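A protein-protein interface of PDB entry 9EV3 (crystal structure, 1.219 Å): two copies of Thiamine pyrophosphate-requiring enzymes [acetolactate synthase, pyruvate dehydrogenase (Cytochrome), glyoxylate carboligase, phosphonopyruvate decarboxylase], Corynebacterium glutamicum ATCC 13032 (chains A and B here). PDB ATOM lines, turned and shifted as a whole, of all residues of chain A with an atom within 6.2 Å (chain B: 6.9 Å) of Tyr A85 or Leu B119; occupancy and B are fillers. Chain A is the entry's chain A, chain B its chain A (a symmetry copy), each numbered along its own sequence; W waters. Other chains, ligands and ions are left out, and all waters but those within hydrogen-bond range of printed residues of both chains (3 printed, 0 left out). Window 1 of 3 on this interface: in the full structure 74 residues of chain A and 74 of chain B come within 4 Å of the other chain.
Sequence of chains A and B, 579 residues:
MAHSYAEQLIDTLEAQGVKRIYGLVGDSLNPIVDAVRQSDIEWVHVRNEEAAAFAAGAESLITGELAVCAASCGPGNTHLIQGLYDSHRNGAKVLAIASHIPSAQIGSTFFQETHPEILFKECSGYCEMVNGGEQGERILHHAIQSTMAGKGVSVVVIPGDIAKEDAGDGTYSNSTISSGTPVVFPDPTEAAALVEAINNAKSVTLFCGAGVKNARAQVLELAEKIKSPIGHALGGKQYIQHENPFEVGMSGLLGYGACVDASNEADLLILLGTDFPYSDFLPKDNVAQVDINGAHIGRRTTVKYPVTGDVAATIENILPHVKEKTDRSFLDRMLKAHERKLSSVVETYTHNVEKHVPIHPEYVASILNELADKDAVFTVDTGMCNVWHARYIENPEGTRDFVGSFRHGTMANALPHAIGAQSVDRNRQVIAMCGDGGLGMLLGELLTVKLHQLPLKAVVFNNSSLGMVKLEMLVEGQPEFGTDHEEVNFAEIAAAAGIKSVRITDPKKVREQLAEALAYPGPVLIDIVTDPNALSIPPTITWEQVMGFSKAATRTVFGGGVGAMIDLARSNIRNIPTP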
ATOM      1  N   LEU A  80     -10.362  -9.686  -6.082  1.00  0.00           N
ATOM      2  CA  LEU A  80     -10.023 -11.041  -5.649  1.00  0.00           C
ATOM      3  C   LEU A  80     -11.174 -12.007  -5.859  1.00  0.00           C
ATOM      4  O   LEU A  80     -10.934 -13.202  -5.815  1.00  0.00           O
ATOM      5  CB  LEU A  80      -9.667 -11.062  -4.132  1.00  0.00           C
ATOM      6  CG  LEU A  80      -8.442 -10.234  -3.729  1.00  0.00           C
ATOM      7  CD1 LEU A  80      -8.401 -10.121  -2.205  1.00  0.00           C
ATOM      8  CD2 LEU A  80      -7.154 -10.917  -4.212  1.00  0.00           C
ATOM      9  N   ILE A  81     -12.437 -11.522  -5.919  1.00  0.00           N
ATOM     10  CA  ILE A  81     -13.579 -12.360  -5.612  1.00  0.00           C
ATOM     11  C   ILE A  81     -13.719 -13.624  -6.454  1.00  0.00           C
ATOM     12  O   ILE A  81     -14.002 -14.686  -5.857  1.00  0.00           O
ATOM     13  CB  ILE A  81     -14.844 -11.518  -5.622  1.00  0.00           C
ATOM     14  CG1 ILE A  81     -15.938 -12.281  -4.863  1.00  0.00           C
ATOM     15  CG2 ILE A  81     -15.258 -11.105  -7.016  1.00  0.00           C
ATOM     16  CD1 ILE A  81     -17.145 -11.377  -4.501  1.00  0.00           C
ATOM     17  N   GLN A  82     -13.458 -13.602  -7.765  1.00  0.00           N
ATOM     18  CA  GLN A  82     -13.659 -14.835  -8.521  1.00  0.00           C
ATOM     19  C   GLN A  82     -12.739 -15.927  -8.054  1.00  0.00           C
ATOM     20  O   GLN A  82     -13.096 -17.098  -7.980  1.00  0.00           O
ATOM     21  CB  GLN A  82     -13.442 -14.574 -10.012  1.00  0.00           C
ATOM     22  CG  GLN A  82     -13.897 -15.764 -10.892  1.00  0.00           C
ATOM     23  CD  GLN A  82     -15.372 -15.645 -11.154  1.00  0.00           C
ATOM     24  OE1 GLN A  82     -16.200 -15.985 -10.318  1.00  0.00           O
ATOM     25  NE2 GLN A  82     -15.717 -15.081 -12.329  1.00  0.00           N
ATOM     26  N   GLY A  83     -11.479 -15.535  -7.758  1.00  0.00           N
ATOM     27  CA  GLY A  83     -10.481 -16.517  -7.316  1.00  0.00           C
ATOM     28  C   GLY A  83     -10.728 -16.996  -5.901  1.00  0.00           C
ATOM     29  O   GLY A  83     -10.314 -18.111  -5.523  1.00  0.00           O
ATOM     30  N   LEU A  84     -11.367 -16.146  -5.096  1.00  0.00           N
ATOM     31  CA  LEU A  84     -11.733 -16.606  -3.736  1.00  0.00           C
ATOM     32  C   LEU A  84     -12.868 -17.620  -3.798  1.00  0.00           C
ATOM     33  O   LEU A  84     -12.837 -18.634  -3.103  1.00  0.00           O
ATOM     34  CB  LEU A  84     -12.115 -15.442  -2.804  1.00  0.00           C
ATOM     35  CG  LEU A  84     -10.967 -14.450  -2.564  1.00  0.00           C
ATOM     36  CD1 LEU A  84     -11.422 -13.381  -1.556  1.00  0.00           C
ATOM     37  CD2 LEU A  84      -9.706 -15.134  -2.075  1.00  0.00           C
ATOM     38  N   TYR A  85     -13.902 -17.365  -4.646  1.00  0.00           N
ATOM     39  CA  TYR A  85     -14.930 -18.410  -4.796  1.00  0.00           C
ATOM     40  C   TYR A  85     -14.299 -19.716  -5.255  1.00  0.00           C
ATOM     41  O   TYR A  85     -14.649 -20.772  -4.748  1.00  0.00           O
ATOM     42  CB  TYR A  85     -15.982 -17.983  -5.846  1.00  0.00           C
ATOM     43  CG  TYR A  85     -17.154 -17.213  -5.291  1.00  0.00           C
ATOM     44  CD1 TYR A  85     -18.208 -17.858  -4.674  1.00  0.00           C
ATOM     45  CD2 TYR A  85     -17.195 -15.828  -5.373  1.00  0.00           C
ATOM     46  CE1 TYR A  85     -19.304 -17.136  -4.174  1.00  0.00           C
ATOM     47  CE2 TYR A  85     -18.297 -15.096  -4.902  1.00  0.00           C
ATOM     48  CZ  TYR A  85     -19.327 -15.752  -4.281  1.00  0.00           C
ATOM     49  OH  TYR A  85     -20.372 -15.008  -3.785  1.00  0.00           O
ATOM     50  N   ASP A  86     -13.407 -19.644  -6.256  1.00  0.00           N
ATOM     51  CA  ASP A  86     -12.826 -20.898  -6.755  1.00  0.00           C
ATOM     52  C   ASP A  86     -12.019 -21.611  -5.671  1.00  0.00           C
ATOM     53  O   ASP A  86     -12.167 -22.823  -5.479  1.00  0.00           O
ATOM     54  CB  ASP A  86     -11.972 -20.610  -7.986  1.00  0.00           C
ATOM     55  CG  ASP A  86     -11.492 -21.885  -8.586  1.00  0.00           C
ATOM     56  OD1 ASP A  86     -12.358 -22.673  -9.062  1.00  0.00           O
ATOM     57  OD2 ASP A  86     -10.261 -22.179  -8.476  1.00  0.00           O
ATOM     58  N   SER A  87     -11.150 -20.837  -4.976  1.00  0.00           N
ATOM     59  CA  SER A  87     -10.337 -21.449  -3.936  1.00  0.00           C
ATOM     60  C   SER A  87     -11.193 -22.016  -2.814  1.00  0.00           C
ATOM     61  O   SER A  87     -10.869 -23.090  -2.250  1.00  0.00           O
ATOM     62  CB  SER A  87      -9.413 -20.381  -3.339  1.00  0.00           C
ATOM     63  OG  SER A  87      -8.486 -19.921  -4.313  1.00  0.00           O
ATOM     64  N   HIS A  88     -12.272 -21.315  -2.479  1.00  0.00           N
ATOM     65  CA  HIS A  88     -13.148 -21.761  -1.396  1.00  0.00           C
ATOM     66  C   HIS A  88     -13.858 -23.036  -1.774  1.00  0.00           C
ATOM     67  O   HIS A  88     -13.870 -24.015  -1.003  1.00  0.00           O
ATOM     68  CB  HIS A  88     -14.155 -20.639  -1.075  1.00  0.00           C
ATOM     69  CG  HIS A  88     -14.995 -20.940   0.104  1.00  0.00           C
ATOM     70  ND1 HIS A  88     -14.459 -21.102   1.373  1.00  0.00           N
ATOM     71  CD2 HIS A  88     -16.324 -21.133   0.153  1.00  0.00           C
ATOM     72  CE1 HIS A  88     -15.500 -21.362   2.166  1.00  0.00           C
ATOM     73  NE2 HIS A  88     -16.646 -21.372   1.490  1.00  0.00           N
ATOM     74  N   ARG A  89     -14.420 -23.093  -2.991  1.00  0.00           N
ATOM     75  CA  ARG A  89     -15.080 -24.328  -3.416  1.00  0.00           C
ATOM     76  C   ARG A  89     -14.126 -25.488  -3.514  1.00  0.00           C
ATOM     77  O   ARG A  89     -14.510 -26.625  -3.240  1.00  0.00           O
ATOM     78  CB  ARG A  89     -15.809 -24.162  -4.758  1.00  0.00           C
ATOM     79  CG  ARG A  89     -16.939 -23.124  -4.783  1.00  0.00           C
ATOM     80  CD  ARG A  89     -18.205 -23.580  -4.062  1.00  0.00           C
ATOM     81  NE  ARG A  89     -18.712 -24.906  -4.462  1.00  0.00           N
ATOM     82  CZ  ARG A  89     -19.621 -25.185  -5.422  1.00  0.00           C
ATOM     83  NH1 ARG A  89     -20.023 -24.256  -6.258  1.00  0.00           N
ATOM     84  NH2 ARG A  89     -20.071 -26.417  -5.578  1.00  0.00           N
ATOM     85  N   ASN A  90     -12.855 -25.229  -3.859  1.00  0.00           N
ATOM     86  CA  ASN A  90     -11.858 -26.284  -3.939  1.00  0.00           C
ATOM     87  C   ASN A  90     -11.242 -26.681  -2.602  1.00  0.00           C
ATOM     88  O   ASN A  90     -10.438 -27.603  -2.609  1.00  0.00           O
ATOM     89  CB  ASN A  90     -10.726 -25.850  -4.895  1.00  0.00           C
ATOM     90  CG  ASN A  90     -11.157 -25.804  -6.345  1.00  0.00           C
ATOM     91  OD1 ASN A  90     -12.172 -26.402  -6.761  1.00  0.00           O
ATOM     92  ND2 ASN A  90     -10.321 -25.162  -7.163  1.00  0.00           N
ATOM     93  N   LEU A 119     -19.186  -8.382   1.774  1.00  0.00           N
ATOM     94  CA  LEU A 119     -19.184  -8.924   0.413  1.00  0.00           C
ATOM     95  C   LEU A 119     -18.650 -10.335   0.352  1.00  0.00           C
ATOM     96  O   LEU A 119     -19.186 -11.140  -0.437  1.00  0.00           O
ATOM     97  CB  LEU A 119     -18.290  -8.005  -0.429  1.00  0.00           C
ATOM     98  CG  LEU A 119     -18.268  -8.302  -1.944  1.00  0.00           C
ATOM     99  CD1 LEU A 119     -19.636  -7.973  -2.559  1.00  0.00           C
ATOM    100  CD2 LEU A 119     -17.143  -7.504  -2.642  1.00  0.00           C
ATOM    101  N   PHE A 120     -17.600 -10.635   1.133  1.00  0.00           N
ATOM    102  CA  PHE A 120     -16.959 -11.947   0.981  1.00  0.00           C
ATOM    103  C   PHE A 120     -17.492 -13.028   1.863  1.00  0.00           C
ATOM    104  O   PHE A 120     -16.911 -14.121   1.907  1.00  0.00           O
ATOM    105  CB  PHE A 120     -15.453 -11.773   1.243  1.00  0.00           C
ATOM    106  CG  PHE A 120     -14.732 -10.907   0.225  1.00  0.00           C
ATOM    107  CD1 PHE A 120     -14.898 -11.109  -1.118  1.00  0.00           C
ATOM    108  CD2 PHE A 120     -13.930  -9.857   0.622  1.00  0.00           C
ATOM    109  CE1 PHE A 120     -14.179 -10.346  -2.053  1.00  0.00           C
ATOM    110  CE2 PHE A 120     -13.227  -9.096  -0.308  1.00  0.00           C
ATOM    111  CZ  PHE A 120     -13.368  -9.345  -1.621  1.00  0.00           C
ATOM    112  N   GLU A 122     -19.969 -15.169   1.297  1.00  0.00           N
ATOM    113  CA  GLU A 122     -20.324 -16.457   0.673  1.00  0.00           C
ATOM    114  C   GLU A 122     -19.090 -17.256   0.224  1.00  0.00           C
ATOM    115  O   GLU A 122     -19.134 -18.504   0.162  1.00  0.00           O
ATOM    116  CB  GLU A 122     -21.243 -16.207  -0.525  1.00  0.00           C
ATOM    117  CG  GLU A 122     -21.757 -17.499  -1.153  1.00  0.00           C
ATOM    118  CD  GLU A 122     -22.667 -17.359  -2.363  1.00  0.00           C
ATOM    119  OE1 GLU A 122     -23.341 -18.386  -2.663  1.00  0.00           O
ATOM    120  OE2 GLU A 122     -22.676 -16.294  -3.047  1.00  0.00           O
ATOM    121  N   CYS A 123     -17.998 -16.545  -0.104  1.00  0.00           N
ATOM    122  CA  CYS A 123     -16.785 -17.220  -0.598  1.00  0.00           C
ATOM    123  C   CYS A 123     -15.733 -17.401   0.473  1.00  0.00           C
ATOM    124  O   CYS A 123     -14.549 -17.465   0.144  1.00  0.00           O
ATOM    125  CB  CYS A 123     -16.213 -16.486  -1.809  1.00  0.00           C
ATOM    126  SG  CYS A 123     -15.690 -14.764  -1.483  1.00  0.00           S
ATOM    127  N   VAL A 153     -11.702 -20.647   2.525  1.00  0.00           N
ATOM    128  CA  VAL A 153     -10.975 -19.376   2.508  1.00  0.00           C
ATOM    129  C   VAL A 153     -11.251 -18.538   3.736  1.00  0.00           C
ATOM    130  O   VAL A 153     -12.353 -18.489   4.254  1.00  0.00           O
ATOM    131  CB  VAL A 153     -11.403 -18.616   1.232  1.00  0.00           C
ATOM    132  CG1 VAL A 153     -11.053 -17.114   1.288  1.00  0.00           C
ATOM    133  CG2 VAL A 153     -10.797 -19.269  -0.017  1.00  0.00           C
ATOM    134  N   HIS A 408     -16.572 -24.423  -8.822  1.00  0.00           N
ATOM    135  CA  HIS A 408     -17.078 -23.091  -9.118  1.00  0.00           C
ATOM    136  C   HIS A 408     -17.280 -22.938 -10.638  1.00  0.00           C
ATOM    137  O   HIS A 408     -18.102 -22.097 -11.048  1.00  0.00           O
ATOM    138  CB  HIS A 408     -16.062 -22.057  -8.570  1.00  0.00           C
ATOM    139  CG  HIS A 408     -16.515 -20.625  -8.725  1.00  0.00           C
ATOM    140  ND1 HIS A 408     -17.746 -20.212  -8.262  1.00  0.00           N
ATOM    141  CD2 HIS A 408     -15.830 -19.554  -9.212  1.00  0.00           C
ATOM    142  CE1 HIS A 408     -17.810 -18.904  -8.517  1.00  0.00           C
ATOM    143  NE2 HIS A 408     -16.674 -18.454  -9.105  1.00  0.00           N
ATOM    144  N   GLY B  74     -23.403 -17.860 -12.013  1.00  0.00           N
ATOM    145  CA  GLY B  74     -22.283 -18.064 -11.111  1.00  0.00           C
ATOM    146  C   GLY B  74     -21.106 -17.175 -11.396  1.00  0.00           C
ATOM    147  O   GLY B  74     -21.198 -15.942 -11.326  1.00  0.00           O
ATOM    148  N   ASN B  77     -21.731 -13.837 -13.930  1.00  0.00           N
ATOM    149  CA  ASN B  77     -22.215 -12.560 -13.388  1.00  0.00           C
ATOM    150  C   ASN B  77     -21.325 -12.048 -12.260  1.00  0.00           C
ATOM    151  O   ASN B  77     -21.224 -10.832 -12.085  1.00  0.00           O
ATOM    152  CB  ASN B  77     -23.713 -12.675 -12.979  1.00  0.00           C
ATOM    153  CG  ASN B  77     -23.968 -13.520 -11.778  1.00  0.00           C
ATOM    154  OD1 ASN B  77     -23.482 -13.214 -10.702  1.00  0.00           O
ATOM    155  ND2 ASN B  77     -24.748 -14.630 -11.918  1.00  0.00           N
ATOM    156  N   THR B  78     -20.570 -12.929 -11.595  1.00  0.00           N
ATOM    157  CA  THR B  78     -19.618 -12.457 -10.574  1.00  0.00           C
ATOM    158  C   THR B  78     -18.640 -11.469 -11.174  1.00  0.00           C
ATOM    159  O   THR B  78     -18.270 -10.484 -10.494  1.00  0.00           O
ATOM    160  CB  THR B  78     -18.928 -13.673  -9.939  1.00  0.00           C
ATOM    161  OG1 THR B  78     -19.926 -14.510  -9.322  1.00  0.00           O
ATOM    162  CG2 THR B  78     -17.961 -13.252  -8.805  1.00  0.00           C
ATOM    163  N   ILE B  81     -18.960  -7.441 -11.183  1.00  0.00           N
ATOM    164  CA  ILE B  81     -19.064  -6.644  -9.977  1.00  0.00           C
ATOM    165  C   ILE B  81     -18.245  -5.358  -9.959  1.00  0.00           C
ATOM    166  O   ILE B  81     -18.805  -4.324  -9.533  1.00  0.00           O
ATOM    167  CB  ILE B  81     -18.790  -7.520  -8.765  1.00  0.00           C
ATOM    168  CG1 ILE B  81     -19.345  -6.810  -7.522  1.00  0.00           C
ATOM    169  CG2 ILE B  81     -17.332  -7.898  -8.638  1.00  0.00           C
ATOM    170  CD1 ILE B  81     -19.445  -7.757  -6.298  1.00  0.00           C
ATOM    171  N   TYR B  85     -20.083  -1.683  -9.314  1.00  0.00           N
ATOM    172  CA  TYR B  85     -19.767  -0.662  -8.301  1.00  0.00           C
ATOM    173  C   TYR B  85     -19.472   0.674  -8.965  1.00  0.00           C
ATOM    174  O   TYR B  85     -19.930   1.704  -8.491  1.00  0.00           O
ATOM    175  CB  TYR B  85     -18.524  -1.083  -7.483  1.00  0.00           C
ATOM    176  CG  TYR B  85     -18.822  -1.901  -6.251  1.00  0.00           C
ATOM    177  CD1 TYR B  85     -19.242  -1.304  -5.079  1.00  0.00           C
ATOM    178  CD2 TYR B  85     -18.697  -3.283  -6.271  1.00  0.00           C
ATOM    179  CE1 TYR B  85     -19.504  -2.071  -3.932  1.00  0.00           C
ATOM    180  CE2 TYR B  85     -18.928  -4.059  -5.125  1.00  0.00           C
ATOM    181  CZ  TYR B  85     -19.357  -3.450  -3.974  1.00  0.00           C
ATOM    182  OH  TYR B  85     -19.625  -4.238  -2.878  1.00  0.00           O
ATOM    183  N   GLU B 113     -22.761 -22.610  -8.253  1.00  0.00           N
ATOM    184  CA  GLU B 113     -23.730 -21.850  -7.469  1.00  0.00           C
ATOM    185  C   GLU B 113     -23.080 -20.678  -6.743  1.00  0.00           C
ATOM    186  O   GLU B 113     -22.042 -20.790  -6.063  1.00  0.00           O
ATOM    187  CB  GLU B 113     -24.399 -22.812  -6.492  1.00  0.00           C
ATOM    188  CG  GLU B 113     -25.497 -22.096  -5.676  1.00  0.00           C
ATOM    189  CD  GLU B 113     -26.474 -22.989  -4.923  1.00  0.00           C
ATOM    190  OE1 GLU B 113     -27.420 -22.450  -4.277  1.00  0.00           O
ATOM    191  OE2 GLU B 113     -26.334 -24.238  -5.032  1.00  0.00           O
ATOM    192  N   THR B 114     -23.781 -19.521  -6.846  1.00  0.00           N
ATOM    193  CA  THR B 114     -23.543 -18.330  -6.037  1.00  0.00           C
ATOM    194  C   THR B 114     -24.934 -17.783  -5.667  1.00  0.00           C
ATOM    195  O   THR B 114     -25.951 -18.320  -6.149  1.00  0.00           O
ATOM    196  CB  THR B 114     -22.725 -17.245  -6.813  1.00  0.00           C
ATOM    197  OG1 THR B 114     -23.503 -16.774  -7.920  1.00  0.00           O
ATOM    198  CG2 THR B 114     -21.373 -17.719  -7.345  1.00  0.00           C
ATOM    199  N   HIS B 115     -24.995 -16.691  -4.869  1.00  0.00           N
ATOM    200  CA  HIS B 115     -26.264 -16.013  -4.563  1.00  0.00           C
ATOM    201  C   HIS B 115     -26.127 -14.550  -5.030  1.00  0.00           C
ATOM    202  O   HIS B 115     -25.871 -13.686  -4.188  1.00  0.00           O
ATOM    203  CB  HIS B 115     -26.606 -16.076  -3.066  1.00  0.00           C
ATOM    204  CG  HIS B 115     -27.003 -17.473  -2.602  1.00  0.00           C
ATOM    205  ND1 HIS B 115     -26.066 -18.493  -2.450  1.00  0.00           N
ATOM    206  CD2 HIS B 115     -28.212 -17.937  -2.182  1.00  0.00           C
ATOM    207  CE1 HIS B 115     -26.735 -19.565  -2.005  1.00  0.00           C
ATOM    208  NE2 HIS B 115     -28.023 -19.279  -1.786  1.00  0.00           N
ATOM    209  N   PRO B 116     -26.278 -14.265  -6.329  1.00  0.00           N
ATOM    210  CA  PRO B 116     -26.061 -12.883  -6.816  1.00  0.00           C
ATOM    211  C   PRO B 116     -27.034 -11.892  -6.215  1.00  0.00           C
ATOM    212  O   PRO B 116     -26.696 -10.747  -6.003  1.00  0.00           O
ATOM    213  CB  PRO B 116     -26.248 -12.970  -8.350  1.00  0.00           C
ATOM    214  CG  PRO B 116     -26.436 -14.418  -8.664  1.00  0.00           C
ATOM    215  CD  PRO B 116     -26.622 -15.207  -7.408  1.00  0.00           C
ATOM    216  N   GLU B 117     -28.237 -12.389  -5.876  1.00  0.00           N
ATOM    217  CA  GLU B 117     -29.258 -11.513  -5.291  1.00  0.00           C
ATOM    218  C   GLU B 117     -28.835 -11.037  -3.919  1.00  0.00           C
ATOM    219  O   GLU B 117     -29.370 -10.009  -3.450  1.00  0.00           O
ATOM    220  CB  GLU B 117     -30.620 -12.240  -5.270  1.00  0.00           C
ATOM    221  CG  GLU B 117     -30.680 -13.446  -4.329  1.00  0.00           C
ATOM    222  CD  GLU B 117     -30.019 -14.750  -4.738  1.00  0.00           C
ATOM    223  OE1 GLU B 117     -30.077 -15.702  -3.944  1.00  0.00           O
ATOM    224  OE2 GLU B 117     -29.399 -14.819  -5.817  1.00  0.00           O
ATOM    225  N   ILE B 118     -27.843 -11.708  -3.255  1.00  0.00           N
ATOM    226  CA  ILE B 118     -27.270 -11.200  -2.016  1.00  0.00           C
ATOM    227  C   ILE B 118     -25.967 -10.457  -2.302  1.00  0.00           C
ATOM    228  O   ILE B 118     -25.723  -9.362  -1.782  1.00  0.00           O
ATOM    229  CB  ILE B 118     -27.004 -12.385  -1.063  1.00  0.00           C
ATOM    230  CG1 ILE B 118     -28.322 -13.098  -0.746  1.00  0.00           C
ATOM    231  CG2 ILE B 118     -26.266 -11.875   0.183  1.00  0.00           C
ATOM    232  CD1 ILE B 118     -28.097 -14.364   0.257  1.00  0.00           C
ATOM    233  N   LEU B 119     -25.130 -11.006  -3.194  1.00  0.00           N
ATOM    234  CA  LEU B 119     -23.810 -10.421  -3.438  1.00  0.00           C
ATOM    235  C   LEU B 119     -23.890  -8.995  -3.928  1.00  0.00           C
ATOM    236  O   LEU B 119     -23.034  -8.179  -3.527  1.00  0.00           O
ATOM    237  CB  LEU B 119     -23.130 -11.287  -4.505  1.00  0.00           C
ATOM    238  CG  LEU B 119     -21.656 -10.942  -4.807  1.00  0.00           C
ATOM    239  CD1 LEU B 119     -20.782 -11.287  -3.592  1.00  0.00           C
ATOM    240  CD2 LEU B 119     -21.167 -11.687  -6.069  1.00  0.00           C
ATOM    241  N   PHE B 120     -24.864  -8.692  -4.799  1.00  0.00           N
ATOM    242  CA  PHE B 120     -24.874  -7.359  -5.415  1.00  0.00           C
ATOM    243  C   PHE B 120     -25.666  -6.322  -4.689  1.00  0.00           C
ATOM    244  O   PHE B 120     -25.849  -5.216  -5.215  1.00  0.00           O
ATOM    245  CB  PHE B 120     -25.414  -7.501  -6.848  1.00  0.00           C
ATOM    246  CG  PHE B 120     -24.531  -8.315  -7.778  1.00  0.00           C
ATOM    247  CD1 PHE B 120     -23.187  -8.074  -7.864  1.00  0.00           C
ATOM    248  CD2 PHE B 120     -25.047  -9.356  -8.522  1.00  0.00           C
ATOM    249  CE1 PHE B 120     -22.388  -8.787  -8.773  1.00  0.00           C
ATOM    250  CE2 PHE B 120     -24.249 -10.067  -9.415  1.00  0.00           C
ATOM    251  CZ  PHE B 120     -22.940  -9.780  -9.518  1.00  0.00           C
ATOM    252  N   LYS B 121     -25.977  -6.556  -3.421  1.00  0.00           N
ATOM    253  CA  LYS B 121     -26.748  -5.535  -2.686  1.00  0.00           C
ATOM    254  C   LYS B 121     -26.017  -4.231  -2.516  1.00  0.00           C
ATOM    255  O   LYS B 121     -26.673  -3.157  -2.620  1.00  0.00           O
ATOM    256  CB  LYS B 121     -27.142  -6.064  -1.291  1.00  0.00           C
ATOM    257  CG  LYS B 121     -28.232  -7.124  -1.382  1.00  0.00           C
ATOM    258  CD  LYS B 121     -29.677  -6.535  -1.427  1.00  0.00           C
ATOM    259  CE  LYS B 121     -30.312  -6.089  -2.711  1.00  0.00           C
ATOM    260  NZ  LYS B 121     -31.425  -5.061  -2.521  1.00  0.00           N
ATOM    261  N   GLU B 122     -24.692  -4.230  -2.298  1.00  0.00           N
ATOM    262  CA  GLU B 122     -24.046  -2.932  -2.028  1.00  0.00           C
ATOM    263  C   GLU B 122     -23.863  -2.087  -3.298  1.00  0.00           C
ATOM    264  O   GLU B 122     -23.827  -0.839  -3.227  1.00  0.00           O
ATOM    265  CB  GLU B 122     -22.688  -3.168  -1.363  1.00  0.00           C
ATOM    266  CG  GLU B 122     -22.007  -1.870  -0.937  1.00  0.00           C
ATOM    267  CD  GLU B 122     -20.641  -1.995  -0.279  1.00  0.00           C
ATOM    268  OE1 GLU B 122     -20.245  -0.977   0.357  1.00  0.00           O
ATOM    269  OE2 GLU B 122     -19.941  -3.038  -0.435  1.00  0.00           O
ATOM    270  N   CYS B 123     -23.731  -2.757  -4.455  1.00  0.00           N
ATOM    271  CA  CYS B 123     -23.498  -2.035  -5.717  1.00  0.00           C
ATOM    272  C   CYS B 123     -24.755  -1.861  -6.539  1.00  0.00           C
ATOM    273  O   CYS B 123     -24.661  -1.754  -7.762  1.00  0.00           O
ATOM    274  CB  CYS B 123     -22.399  -2.714  -6.534  1.00  0.00           C
ATOM    275  SG  CYS B 123     -22.775  -4.431  -7.040  1.00  0.00           S
ATOM    276  N   CYS B 127     -32.128  -5.076  -6.450  1.00  0.00           N
ATOM    277  CA  CYS B 127     -31.481  -6.323  -6.750  1.00  0.00           C
ATOM    278  C   CYS B 127     -32.388  -7.434  -6.235  1.00  0.00           C
ATOM    279  O   CYS B 127     -32.533  -7.589  -5.005  1.00  0.00           O
ATOM    280  CB  CYS B 127     -30.115  -6.330  -6.053  1.00  0.00           C
ATOM    281  SG  CYS B 127     -29.190  -7.887  -6.283  1.00  0.00           S
HETATM  282  O   HOH W   1     -20.985 -20.713  -3.456  1.00  0.00           O
HETATM  283  O   HOH W   2     -23.553 -13.781  -1.735  1.00  0.00           O
HETATM  284  O   HOH W   3     -19.598 -21.761  -6.919  1.00  0.00           O
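A ring nitrogen (ND1) of His B115 lies within hydrogen-bond range of the side-chain carboxylate of Glu A122 (2.7 Å).
OE1 of Gln A82 is in hydrogen-bond range of NE2 of His A408 (2.8 Å).
The side-chain hydroxyl (OH) of Tyr A85 sits at hydrogen-bond distance from the side-chain carboxylate (OE2) of Glu A122, at 2.7 Å.
OG1 of Thr B78 is in hydrogen-bond range of O of Gly B74 (2.8 Å).
The side-chain hydroxyl (OH) of Tyr B85 lies within hydrogen-bond range of the side-chain carboxylate (OE2) of Glu B122.
Ile A81 touches Thr B78.
Leu B119 touches Ile A81 (CD1 to CD1, 3.7 Å).
Gln A82 touches Thr B78.
Tyr A85 touches Thr B114.
Leu B119 touches Tyr A85 (CD1 to OH, 3.7 Å).
Arg A89 touches Glu B113.
CD1 of Leu A119 touches OH of Tyr B85 (3.7 Å).
Leu B119 touches Leu A119 (CD1 to O, 3.5 Å).
Glu A122 touches Thr B114.
Thr B114 touches His A408 (CG2 to CE1, 3.9 Å).
Printed residues of chain B within 4 Å of Gln A82: Thr B78 (3.6 Å).
Of chain B, only Thr B114 (3.8 Å) and Leu B119 (3.7 Å) come within 4 Å of Tyr A85.
Asn A90 touches none of the printed residues of chain B.
Val A153 touches none of the printed residues of chain B.
Of the printed residues of chain A, Glu B113 touches Arg A89 (3.8 Å).
Printed residues of chain A that touch a printed residue of chain B: Ile A81, Gln A82, Tyr A85, Arg A89, Leu A119, Glu A122 and His A408.
Hydrophobic or aromatic side chains of chain A that line the printed part of chain B: Ile A81, Tyr A85, Leu A119 and His A408.
Hydrophobic or aromatic side chains of chain B that line the printed part of chain A: Ile B81, Tyr B85, His B115 and Leu B119.
Among the printed residues, no Asp or Glu carboxylate lies within 4 Å of a Lys or Arg side-chain nitrogen of the other chain.
Ile A81 touches Leu B119, and with the chains exchanged Leu A119 touches Ile B81.
Tyr A85 touches Leu B119, and with the chains exchanged Leu A119 touches Tyr B85.
Leu A119 touches its own counterpart, Leu B119.
6 positions are printed for both chains.
Water W3 lies within hydrogen-bond range of the guanidinium group of Arg A89 (2.6 Å), a ring nitrogen (ND1) of His A408 (2.8 Å) and the backbone carbonyl oxygen of Glu B113 (2.8 Å).
Water W1 lies within hydrogen-bond range of the backbone carbonyl oxygen (O) of Glu B113 and the side-chain carboxylate (OE1) of Glu A122.
Water W2 bridges the side-chain carboxylate of Glu A122 and the backbone carbonyl oxygen of His B115.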
